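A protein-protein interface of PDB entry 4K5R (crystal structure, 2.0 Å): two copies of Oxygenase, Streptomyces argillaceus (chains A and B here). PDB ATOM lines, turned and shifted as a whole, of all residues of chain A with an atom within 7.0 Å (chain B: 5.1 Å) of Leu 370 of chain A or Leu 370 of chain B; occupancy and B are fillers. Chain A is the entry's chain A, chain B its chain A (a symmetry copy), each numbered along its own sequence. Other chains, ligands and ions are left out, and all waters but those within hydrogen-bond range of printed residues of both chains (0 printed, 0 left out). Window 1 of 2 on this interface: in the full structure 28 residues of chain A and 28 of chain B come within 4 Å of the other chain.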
ATOM      1  N   PHE A  88      -2.995  -9.735  -6.506  1.00  0.00           N
ATOM      2  CA  PHE A  88      -3.318  -8.313  -6.466  1.00  0.00           C
ATOM      3  C   PHE A  88      -2.135  -7.513  -6.981  1.00  0.00           C
ATOM      4  O   PHE A  88      -1.037  -7.598  -6.425  1.00  0.00           O
ATOM      5  CB  PHE A  88      -3.671  -7.867  -5.047  1.00  0.00           C
ATOM      6  CG  PHE A  88      -3.923  -6.391  -4.920  1.00  0.00           C
ATOM      7  CD1 PHE A  88      -5.098  -5.829  -5.398  1.00  0.00           C
ATOM      8  CD2 PHE A  88      -2.982  -5.560  -4.318  1.00  0.00           C
ATOM      9  CE1 PHE A  88      -5.340  -4.458  -5.277  1.00  0.00           C
ATOM     10  CE2 PHE A  88      -3.211  -4.189  -4.193  1.00  0.00           C
ATOM     11  CZ  PHE A  88      -4.398  -3.638  -4.678  1.00  0.00           C
ATOM     12  N   ILE A  91       0.877  -9.586  -7.642  1.00  0.00           N
ATOM     13  CA  ILE A  91       1.505 -10.248  -6.488  1.00  0.00           C
ATOM     14  C   ILE A  91       0.813 -11.580  -6.200  1.00  0.00           C
ATOM     15  O   ILE A  91      -0.361 -11.608  -5.826  1.00  0.00           O
ATOM     16  CB  ILE A  91       1.473  -9.370  -5.218  1.00  0.00           C
ATOM     17  CG1 ILE A  91       2.348  -8.127  -5.408  1.00  0.00           C
ATOM     18  CG2 ILE A  91       1.953 -10.172  -4.011  1.00  0.00           C
ATOM     19  CD1 ILE A  91       2.121  -7.037  -4.377  1.00  0.00           C
ATOM     20  N   LEU A 351     -10.095   4.613  -9.056  1.00  0.00           N
ATOM     21  CA  LEU A 351      -8.992   4.877  -8.143  1.00  0.00           C
ATOM     22  C   LEU A 351      -8.143   3.631  -7.908  1.00  0.00           C
ATOM     23  O   LEU A 351      -6.918   3.722  -7.896  1.00  0.00           O
ATOM     24  CB  LEU A 351      -9.503   5.444  -6.810  1.00  0.00           C
ATOM     25  CG  LEU A 351     -10.084   6.849  -6.969  1.00  0.00           C
ATOM     26  CD1 LEU A 351     -10.728   7.358  -5.680  1.00  0.00           C
ATOM     27  CD2 LEU A 351      -9.010   7.820  -7.477  1.00  0.00           C
ATOM     28  N   ARG A 354      -5.947   2.632 -10.934  1.00  0.00           N
ATOM     29  CA  ARG A 354      -4.849   3.586 -11.017  1.00  0.00           C
ATOM     30  C   ARG A 354      -3.799   3.327  -9.931  1.00  0.00           C
ATOM     31  O   ARG A 354      -2.595   3.353 -10.211  1.00  0.00           O
ATOM     32  CB  ARG A 354      -5.363   5.021 -10.948  1.00  0.00           C
ATOM     33  CG  ARG A 354      -6.316   5.385 -12.063  1.00  0.00           C
ATOM     34  CD  ARG A 354      -6.954   6.745 -11.803  1.00  0.00           C
ATOM     35  NE  ARG A 354      -5.944   7.750 -11.477  1.00  0.00           N
ATOM     36  CZ  ARG A 354      -6.220   8.974 -11.037  1.00  0.00           C
ATOM     37  NH1 ARG A 354      -5.238   9.819 -10.755  1.00  0.00           N
ATOM     38  NH2 ARG A 354      -7.477   9.349 -10.861  1.00  0.00           N
ATOM     39  N   ALA A 355      -4.256   3.074  -8.703  1.00  0.00           N
ATOM     40  CA  ALA A 355      -3.365   2.710  -7.607  1.00  0.00           C
ATOM     41  C   ALA A 355      -2.601   1.420  -7.901  1.00  0.00           C
ATOM     42  O   ALA A 355      -1.415   1.309  -7.588  1.00  0.00           O
ATOM     43  CB  ALA A 355      -4.150   2.573  -6.295  1.00  0.00           C
ATOM     44  N   GLN A 356      -3.276   0.439  -8.492  1.00  0.00           N
ATOM     45  CA  GLN A 356      -2.602  -0.812  -8.820  1.00  0.00           C
ATOM     46  C   GLN A 356      -1.519  -0.570  -9.866  1.00  0.00           C
ATOM     47  O   GLN A 356      -0.423  -1.132  -9.773  1.00  0.00           O
ATOM     48  CB  GLN A 356      -3.586  -1.876  -9.295  1.00  0.00           C
ATOM     49  CG  GLN A 356      -4.463  -2.440  -8.194  1.00  0.00           C
ATOM     50  CD  GLN A 356      -5.312  -3.590  -8.684  1.00  0.00           C
ATOM     51  OE1 GLN A 356      -6.516  -3.432  -8.937  1.00  0.00           O
ATOM     52  NE2 GLN A 356      -4.688  -4.755  -8.843  1.00  0.00           N
ATOM     53  N   ALA A 358       0.308   2.056 -10.164  1.00  0.00           N
ATOM     54  CA  ALA A 358       1.443   2.545  -9.385  1.00  0.00           C
ATOM     55  C   ALA A 358       2.241   1.395  -8.757  1.00  0.00           C
ATOM     56  O   ALA A 358       3.476   1.411  -8.758  1.00  0.00           O
ATOM     57  CB  ALA A 358       0.976   3.519  -8.308  1.00  0.00           C
ATOM     58  N   LEU A 359       1.530   0.397  -8.228  1.00  0.00           N
ATOM     59  CA  LEU A 359       2.176  -0.736  -7.567  1.00  0.00           C
ATOM     60  C   LEU A 359       2.931  -1.661  -8.505  1.00  0.00           C
ATOM     61  O   LEU A 359       3.874  -2.332  -8.084  1.00  0.00           O
ATOM     62  CB  LEU A 359       1.153  -1.565  -6.799  1.00  0.00           C
ATOM     63  CG  LEU A 359       0.917  -1.194  -5.345  1.00  0.00           C
ATOM     64  CD1 LEU A 359      -0.254  -2.002  -4.808  1.00  0.00           C
ATOM     65  CD2 LEU A 359       2.177  -1.454  -4.553  1.00  0.00           C
ATOM     66  N   GLN A 365      14.134   0.601  -8.487  1.00  0.00           N
ATOM     67  CA  GLN A 365      14.722   1.423  -7.497  1.00  0.00           C
ATOM     68  C   GLN A 365      13.807   1.677  -6.315  1.00  0.00           C
ATOM     69  O   GLN A 365      14.256   1.667  -5.211  1.00  0.00           O
ATOM     70  CB  GLN A 365      15.159   2.731  -8.114  1.00  0.00           C
ATOM     71  CG  GLN A 365      15.869   3.689  -7.194  1.00  0.00           C
ATOM     72  CD  GLN A 365      17.386   3.656  -7.321  1.00  0.00           C
ATOM     73  OE1 GLN A 365      18.076   4.541  -6.855  1.00  0.00           O
ATOM     74  NE2 GLN A 365      17.896   2.624  -7.942  1.00  0.00           N
ATOM     75  N   HIS A 366      12.530   1.935  -6.567  1.00  0.00           N
ATOM     76  CA  HIS A 366      11.618   2.236  -5.472  1.00  0.00           C
ATOM     77  C   HIS A 366      10.418   1.292  -5.386  1.00  0.00           C
ATOM     78  O   HIS A 366      10.050   0.855  -4.309  1.00  0.00           O
ATOM     79  CB  HIS A 366      11.122   3.684  -5.570  1.00  0.00           C
ATOM     80  CG  HIS A 366      12.219   4.694  -5.597  1.00  0.00           C
ATOM     81  ND1 HIS A 366      12.228   5.758  -6.475  1.00  0.00           N
ATOM     82  CD2 HIS A 366      13.354   4.801  -4.862  1.00  0.00           C
ATOM     83  CE1 HIS A 366      13.321   6.476  -6.279  1.00  0.00           C
ATOM     84  NE2 HIS A 366      14.017   5.921  -5.304  1.00  0.00           N
ATOM     85  N   THR A 367       9.818   0.981  -6.525  1.00  0.00           N
ATOM     86  CA  THR A 367       8.568   0.242  -6.535  1.00  0.00           C
ATOM     87  C   THR A 367       8.743  -1.229  -6.180  1.00  0.00           C
ATOM     88  O   THR A 367       7.870  -1.833  -5.546  1.00  0.00           O
ATOM     89  CB  THR A 367       7.836   0.435  -7.868  1.00  0.00           C
ATOM     90  OG1 THR A 367       7.628   1.832  -8.049  1.00  0.00           O
ATOM     91  CG2 THR A 367       6.472  -0.258  -7.861  1.00  0.00           C
ATOM     92  N   THR A 368       9.874  -1.809  -6.557  1.00  0.00           N
ATOM     93  CA  THR A 368      10.141  -3.177  -6.129  1.00  0.00           C
ATOM     94  C   THR A 368      10.137  -3.318  -4.588  1.00  0.00           C
ATOM     95  O   THR A 368       9.376  -4.133  -4.058  1.00  0.00           O
ATOM     96  CB  THR A 368      11.394  -3.771  -6.800  1.00  0.00           C
ATOM     97  OG1 THR A 368      11.080  -4.085  -8.166  1.00  0.00           O
ATOM     98  CG2 THR A 368      11.837  -5.038  -6.077  1.00  0.00           C
ATOM     99  N   PRO A 369      10.948  -2.507  -3.868  1.00  0.00           N
ATOM    100  CA  PRO A 369      10.897  -2.494  -2.395  1.00  0.00           C
ATOM    101  C   PRO A 369       9.510  -2.202  -1.841  1.00  0.00           C
ATOM    102  O   PRO A 369       9.125  -2.792  -0.826  1.00  0.00           O
ATOM    103  CB  PRO A 369      11.836  -1.352  -2.022  1.00  0.00           C
ATOM    104  CG  PRO A 369      12.842  -1.358  -3.125  1.00  0.00           C
ATOM    105  CD  PRO A 369      12.030  -1.641  -4.369  1.00  0.00           C
ATOM    106  N   LEU A 370       8.764  -1.309  -2.486  1.00  0.00           N
ATOM    107  CA  LEU A 370       7.414  -1.011  -2.024  1.00  0.00           C
ATOM    108  C   LEU A 370       6.501  -2.242  -2.124  1.00  0.00           C
ATOM    109  O   LEU A 370       5.667  -2.496  -1.234  1.00  0.00           O
ATOM    110  CB  LEU A 370       6.812   0.177  -2.778  1.00  0.00           C
ATOM    111  CG  LEU A 370       5.338   0.425  -2.404  1.00  0.00           C
ATOM    112  CD1 LEU A 370       5.200   0.900  -0.963  1.00  0.00           C
ATOM    113  CD2 LEU A 370       4.701   1.419  -3.342  1.00  0.00           C
ATOM    114  N   ARG A 371       6.666  -3.003  -3.205  1.00  0.00           N
ATOM    115  CA  ARG A 371       5.901  -4.234  -3.402  1.00  0.00           C
ATOM    116  C   ARG A 371       6.202  -5.276  -2.314  1.00  0.00           C
ATOM    117  O   ARG A 371       5.317  -6.022  -1.901  1.00  0.00           O
ATOM    118  CB  ARG A 371       6.142  -4.807  -4.800  1.00  0.00           C
ATOM    119  CG  ARG A 371       5.588  -3.933  -5.917  1.00  0.00           C
ATOM    120  CD  ARG A 371       6.081  -4.397  -7.278  1.00  0.00           C
ATOM    121  NE  ARG A 371       5.623  -5.744  -7.608  1.00  0.00           N
ATOM    122  CZ  ARG A 371       4.390  -6.039  -8.017  1.00  0.00           C
ATOM    123  NH1 ARG A 371       3.477  -5.084  -8.138  1.00  0.00           N
ATOM    124  NH2 ARG A 371       4.065  -7.296  -8.299  1.00  0.00           N
ATOM    125  N   GLY A 372       7.443  -5.313  -1.842  1.00  0.00           N
ATOM    126  CA  GLY A 372       7.795  -6.189  -0.740  1.00  0.00           C
ATOM    127  C   GLY A 372       6.945  -5.936   0.491  1.00  0.00           C
ATOM    128  O   GLY A 372       6.474  -6.873   1.136  1.00  0.00           O
ATOM    129  N   PHE A 373       6.732  -4.664   0.814  1.00  0.00           N
ATOM    130  CA  PHE A 373       5.997  -4.307   2.021  1.00  0.00           C
ATOM    131  C   PHE A 373       4.512  -4.551   1.848  1.00  0.00           C
ATOM    132  O   PHE A 373       3.841  -4.998   2.780  1.00  0.00           O
ATOM    133  CB  PHE A 373       6.283  -2.865   2.449  1.00  0.00           C
ATOM    134  CG  PHE A 373       7.669  -2.675   3.000  1.00  0.00           C
ATOM    135  CD1 PHE A 373       7.950  -2.973   4.326  1.00  0.00           C
ATOM    136  CD2 PHE A 373       8.702  -2.230   2.184  1.00  0.00           C
ATOM    137  CE1 PHE A 373       9.237  -2.820   4.833  1.00  0.00           C
ATOM    138  CE2 PHE A 373       9.996  -2.074   2.684  1.00  0.00           C
ATOM    139  CZ  PHE A 373      10.258  -2.366   4.014  1.00  0.00           C
ATOM    140  N   VAL A 374       3.996  -4.270   0.655  1.00  0.00           N
ATOM    141  CA  VAL A 374       2.599  -4.569   0.381  1.00  0.00           C
ATOM    142  C   VAL A 374       2.326  -6.065   0.507  1.00  0.00           C
ATOM    143  O   VAL A 374       1.298  -6.478   1.058  1.00  0.00           O
ATOM    144  CB  VAL A 374       2.161  -4.102  -1.002  1.00  0.00           C
ATOM    145  CG1 VAL A 374       0.768  -4.638  -1.304  1.00  0.00           C
ATOM    146  CG2 VAL A 374       2.196  -2.585  -1.071  1.00  0.00           C
ATOM    147  N   GLU A 375       3.250  -6.868  -0.004  1.00  0.00           N
ATOM    148  CA  GLU A 375       3.148  -8.314   0.087  1.00  0.00           C
ATOM    149  C   GLU A 375       3.076  -8.811   1.544  1.00  0.00           C
ATOM    150  O   GLU A 375       2.248  -9.663   1.871  1.00  0.00           O
ATOM    151  CB  GLU A 375       4.309  -8.970  -0.654  1.00  0.00           C
ATOM    152  CG  GLU A 375       4.258 -10.480  -0.651  1.00  0.00           C
ATOM    153  CD  GLU A 375       5.351 -11.100  -1.494  1.00  0.00           C
ATOM    154  OE1 GLU A 375       5.773 -12.233  -1.177  1.00  0.00           O
ATOM    155  OE2 GLU A 375       5.784 -10.457  -2.475  1.00  0.00           O
ATOM    156  N   PHE A 387      -8.500  -5.768   0.532  1.00  0.00           N
ATOM    157  CA  PHE A 387      -8.341  -5.776  -0.925  1.00  0.00           C
ATOM    158  C   PHE A 387      -9.236  -6.792  -1.621  1.00  0.00           C
ATOM    159  O   PHE A 387      -9.777  -6.515  -2.698  1.00  0.00           O
ATOM    160  CB  PHE A 387      -6.875  -5.968  -1.301  1.00  0.00           C
ATOM    161  CG  PHE A 387      -6.043  -4.773  -1.000  1.00  0.00           C
ATOM    162  CD1 PHE A 387      -6.257  -3.589  -1.690  1.00  0.00           C
ATOM    163  CD2 PHE A 387      -5.076  -4.810  -0.013  1.00  0.00           C
ATOM    164  CE1 PHE A 387      -5.512  -2.471  -1.415  1.00  0.00           C
ATOM    165  CE2 PHE A 387      -4.322  -3.695   0.267  1.00  0.00           C
ATOM    166  CZ  PHE A 387      -4.539  -2.523  -0.432  1.00  0.00           C
ATOM    167  N   ALA B 355      11.012   2.226  -0.451  1.00  0.00           N
ATOM    168  CA  ALA B 355       9.567   2.077  -0.573  1.00  0.00           C
ATOM    169  C   ALA B 355       8.838   3.400  -0.342  1.00  0.00           C
ATOM    170  O   ALA B 355       7.868   3.711  -1.035  1.00  0.00           O
ATOM    171  CB  ALA B 355       9.048   1.010   0.402  1.00  0.00           C
ATOM    172  N   ALA B 358       8.956   5.562  -3.392  1.00  0.00           N
ATOM    173  CA  ALA B 358       7.910   5.154  -4.327  1.00  0.00           C
ATOM    174  C   ALA B 358       6.558   5.793  -3.982  1.00  0.00           C
ATOM    175  O   ALA B 358       5.830   6.246  -4.872  1.00  0.00           O
ATOM    176  CB  ALA B 358       7.786   3.635  -4.368  1.00  0.00           C
ATOM    177  N   LEU B 359       6.231   5.831  -2.689  1.00  0.00           N
ATOM    178  CA  LEU B 359       4.952   6.379  -2.239  1.00  0.00           C
ATOM    179  C   LEU B 359       4.823   7.883  -2.401  1.00  0.00           C
ATOM    180  O   LEU B 359       3.712   8.398  -2.527  1.00  0.00           O
ATOM    181  CB  LEU B 359       4.703   6.033  -0.776  1.00  0.00           C
ATOM    182  CG  LEU B 359       3.948   4.746  -0.490  1.00  0.00           C
ATOM    183  CD1 LEU B 359       3.961   4.483   1.007  1.00  0.00           C
ATOM    184  CD2 LEU B 359       2.538   4.867  -1.018  1.00  0.00           C
ATOM    185  N   HIS B 366      -0.917   7.853 -11.112  1.00  0.00           N
ATOM    186  CA  HIS B 366      -1.041   6.595 -10.389  1.00  0.00           C
ATOM    187  C   HIS B 366      -0.742   6.707  -8.893  1.00  0.00           C
ATOM    188  O   HIS B 366      -1.453   6.146  -8.076  1.00  0.00           O
ATOM    189  CB  HIS B 366      -0.134   5.527 -11.012  1.00  0.00           C
ATOM    190  CG  HIS B 366      -0.389   5.294 -12.463  1.00  0.00           C
ATOM    191  ND1 HIS B 366       0.630   5.180 -13.387  1.00  0.00           N
ATOM    192  CD2 HIS B 366      -1.546   5.167 -13.158  1.00  0.00           C
ATOM    193  CE1 HIS B 366       0.109   4.991 -14.589  1.00  0.00           C
ATOM    194  NE2 HIS B 366      -1.207   4.974 -14.476  1.00  0.00           N
ATOM    195  N   THR B 367       0.309   7.434  -8.545  1.00  0.00           N
ATOM    196  CA  THR B 367       0.783   7.455  -7.173  1.00  0.00           C
ATOM    197  C   THR B 367      -0.125   8.249  -6.242  1.00  0.00           C
ATOM    198  O   THR B 367      -0.283   7.900  -5.066  1.00  0.00           O
ATOM    199  CB  THR B 367       2.238   7.932  -7.110  1.00  0.00           C
ATOM    200  OG1 THR B 367       3.014   7.059  -7.926  1.00  0.00           O
ATOM    201  CG2 THR B 367       2.785   7.869  -5.682  1.00  0.00           C
ATOM    202  N   THR B 368      -0.747   9.300  -6.759  1.00  0.00           N
ATOM    203  CA  THR B 368      -1.723  10.013  -5.943  1.00  0.00           C
ATOM    204  C   THR B 368      -2.869   9.091  -5.465  1.00  0.00           C
ATOM    205  O   THR B 368      -3.099   8.990  -4.255  1.00  0.00           O
ATOM    206  CB  THR B 368      -2.213  11.312  -6.611  1.00  0.00           C
ATOM    207  OG1 THR B 368      -1.172  12.297  -6.520  1.00  0.00           O
ATOM    208  CG2 THR B 368      -3.465  11.831  -5.913  1.00  0.00           C
ATOM    209  N   PRO B 369      -3.560   8.391  -6.395  1.00  0.00           N
ATOM    210  CA  PRO B 369      -4.572   7.395  -6.001  1.00  0.00           C
ATOM    211  C   PRO B 369      -4.032   6.320  -5.068  1.00  0.00           C
ATOM    212  O   PRO B 369      -4.746   5.895  -4.155  1.00  0.00           O
ATOM    213  CB  PRO B 369      -4.969   6.755  -7.327  1.00  0.00           C
ATOM    214  CG  PRO B 369      -4.785   7.860  -8.314  1.00  0.00           C
ATOM    215  CD  PRO B 369      -3.522   8.559  -7.859  1.00  0.00           C
ATOM    216  N   LEU B 370      -2.795   5.881  -5.286  1.00  0.00           N
ATOM    217  CA  LEU B 370      -2.210   4.876  -4.407  1.00  0.00           C
ATOM    218  C   LEU B 370      -2.056   5.406  -2.972  1.00  0.00           C
ATOM    219  O   LEU B 370      -2.289   4.675  -1.992  1.00  0.00           O
ATOM    220  CB  LEU B 370      -0.870   4.370  -4.947  1.00  0.00           C
ATOM    221  CG  LEU B 370      -0.167   3.410  -3.968  1.00  0.00           C
ATOM    222  CD1 LEU B 370      -0.931   2.100  -3.824  1.00  0.00           C
ATOM    223  CD2 LEU B 370       1.252   3.139  -4.401  1.00  0.00           C
ATOM    224  N   ARG B 371      -1.670   6.676  -2.858  1.00  0.00           N
ATOM    225  CA  ARG B 371      -1.536   7.323  -1.554  1.00  0.00           C
ATOM    226  C   ARG B 371      -2.879   7.402  -0.812  1.00  0.00           C
ATOM    227  O   ARG B 371      -2.926   7.287   0.410  1.00  0.00           O
ATOM    228  CB  ARG B 371      -0.900   8.708  -1.697  1.00  0.00           C
ATOM    229  CG  ARG B 371       0.552   8.663  -2.155  1.00  0.00           C
ATOM    230  CD  ARG B 371       1.053  10.046  -2.539  1.00  0.00           C
ATOM    231  NE  ARG B 371       1.056  10.972  -1.409  1.00  0.00           N
ATOM    232  CZ  ARG B 371       1.969  10.972  -0.440  1.00  0.00           C
ATOM    233  NH1 ARG B 371       2.955  10.085  -0.448  1.00  0.00           N
ATOM    234  NH2 ARG B 371       1.893  11.857   0.547  1.00  0.00           N
ATOM    235  N   GLY B 372      -3.967   7.581  -1.554  1.00  0.00           N
ATOM    236  CA  GLY B 372      -5.288   7.562  -0.954  1.00  0.00           C
ATOM    237  C   GLY B 372      -5.563   6.268  -0.210  1.00  0.00           C
ATOM    238  O   GLY B 372      -6.094   6.280   0.902  1.00  0.00           O
ATOM    239  N   PHE B 373      -5.191   5.144  -0.814  1.00  0.00           N
ATOM    240  CA  PHE B 373      -5.478   3.843  -0.226  1.00  0.00           C
ATOM    241  C   PHE B 373      -4.563   3.559   0.948  1.00  0.00           C
ATOM    242  O   PHE B 373      -4.995   2.987   1.951  1.00  0.00           O
ATOM    243  CB  PHE B 373      -5.413   2.725  -1.271  1.00  0.00           C
ATOM    244  CG  PHE B 373      -6.558   2.757  -2.245  1.00  0.00           C
ATOM    245  CD1 PHE B 373      -7.780   2.186  -1.919  1.00  0.00           C
ATOM    246  CD2 PHE B 373      -6.425   3.390  -3.475  1.00  0.00           C
ATOM    247  CE1 PHE B 373      -8.848   2.234  -2.809  1.00  0.00           C
ATOM    248  CE2 PHE B 373      -7.492   3.444  -4.374  1.00  0.00           C
ATOM    249  CZ  PHE B 373      -8.703   2.859  -4.038  1.00  0.00           C
ATOM    250  N   VAL B 374      -3.303   3.967   0.833  1.00  0.00           N
ATOM    251  CA  VAL B 374      -2.389   3.819   1.956  1.00  0.00           C
ATOM    252  C   VAL B 374      -2.877   4.612   3.165  1.00  0.00           C
ATOM    253  O   VAL B 374      -2.812   4.135   4.305  1.00  0.00           O
ATOM    254  CB  VAL B 374      -0.970   4.259   1.617  1.00  0.00           C
ATOM    255  CG1 VAL B 374      -0.127   4.286   2.884  1.00  0.00           C
ATOM    256  CG2 VAL B 374      -0.373   3.325   0.577  1.00  0.00           C
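Among the printed residues, merely in contact across the chains: Arg 354 of chain A with Pro 369 of chain B (3.2 Å), Arg 354 of chain A with His 366 of chain B (3.4 Å), Ala 358 of chain A with His 366 of chain B (3.5 Å), His 366 of chain A with Ala 358 of chain B (3.5 Å), Ala 355 of chain A with Leu 370 of chain B (3.6 Å), Leu 370 of chain A with Ala 355 of chain B (3.6 Å), Leu 351 of chain A with Phe 373 of chain B (3.6 Å), Leu 351 of chain A with Pro 369 of chain B (3.6 Å), Phe 373 of chain A with Ala 355 of chain B (3.7 Å), Ala 355 of chain A with Phe 373 of chain B (3.7 Å), Ala 358 of chain A with Leu 370 of chain B (3.9 Å), Leu 370 of chain A with Ala 358 of chain B (3.9 Å), Ala 355 of chain A with Pro 369 of chain B (3.9 Å), Pro 369 of chain A with Ala 355 of chain B (3.9 Å), Ala 355 of chain A with His 366 of chain B (3.96 Å), His 366 of chain A with Ala 355 of chain B (3.96 Å), Thr 367 of chain A with Ala 358 of chain B (3.98 Å), Ala 358 of chain A with Thr 367 of chain B (3.98 Å) and Leu 370 of chain A with Leu 370 of chain B (3.997 Å).
Of the printed residues of chain B, Leu 370 of chain A touches Ala 355 (3.6 Å), Ala 358 (3.9 Å) and Leu 370 (3.997 Å). Of the printed residues of chain A, Leu 370 of chain B touches Ala 355, Ala 358 and Leu 370. Of the printed residues of chain B, Leu 351 of chain A touches Pro 369 (3.6 Å) and Phe 373 (3.6 Å). Of the printed residues of chain B, Phe 373 of chain A touches Ala 355 (3.7 Å). Ile 91 of chain A touches none of the printed residues of chain B. Gly 372 of chain A touches none of the printed residues of chain B. The nearest printed residue of chain B that does not touch Leu 370 of chain A is Leu 359 of chain B (4.1 Å). The nearest printed residue of chain A that does not touch Leu 370 of chain B is Leu 359 of chain A (4.1 Å). The nearest printed residue of chain B that does not touch Thr 367 of chain A is Ala 355 of chain B (6.1 Å).
Of the 20 printed residues of chain A, 9 touch a printed residue of chain B. Of the 12 printed residues of chain B, 7 touch a printed residue of chain A. Among the printed residues, no Asp or Glu carboxylate lies within 4 Å of a Lys or Arg side-chain nitrogen of the other chain.
Ala 355 of chain A touches Leu 370 of chain B, and with the chains exchanged Leu 370 of chain A touches Ala 355 of chain B. Ala 355 of chain A touches Phe 373 of chain B, and with the chains exchanged Phe 373 of chain A touches Ala 355 of chain B. Ala 358 of chain A touches His 366 of chain B, and with the chains exchanged His 366 of chain A touches Ala 358 of chain B. Leu 370 of chain A touches its own counterpart, Leu 370 of chain B.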
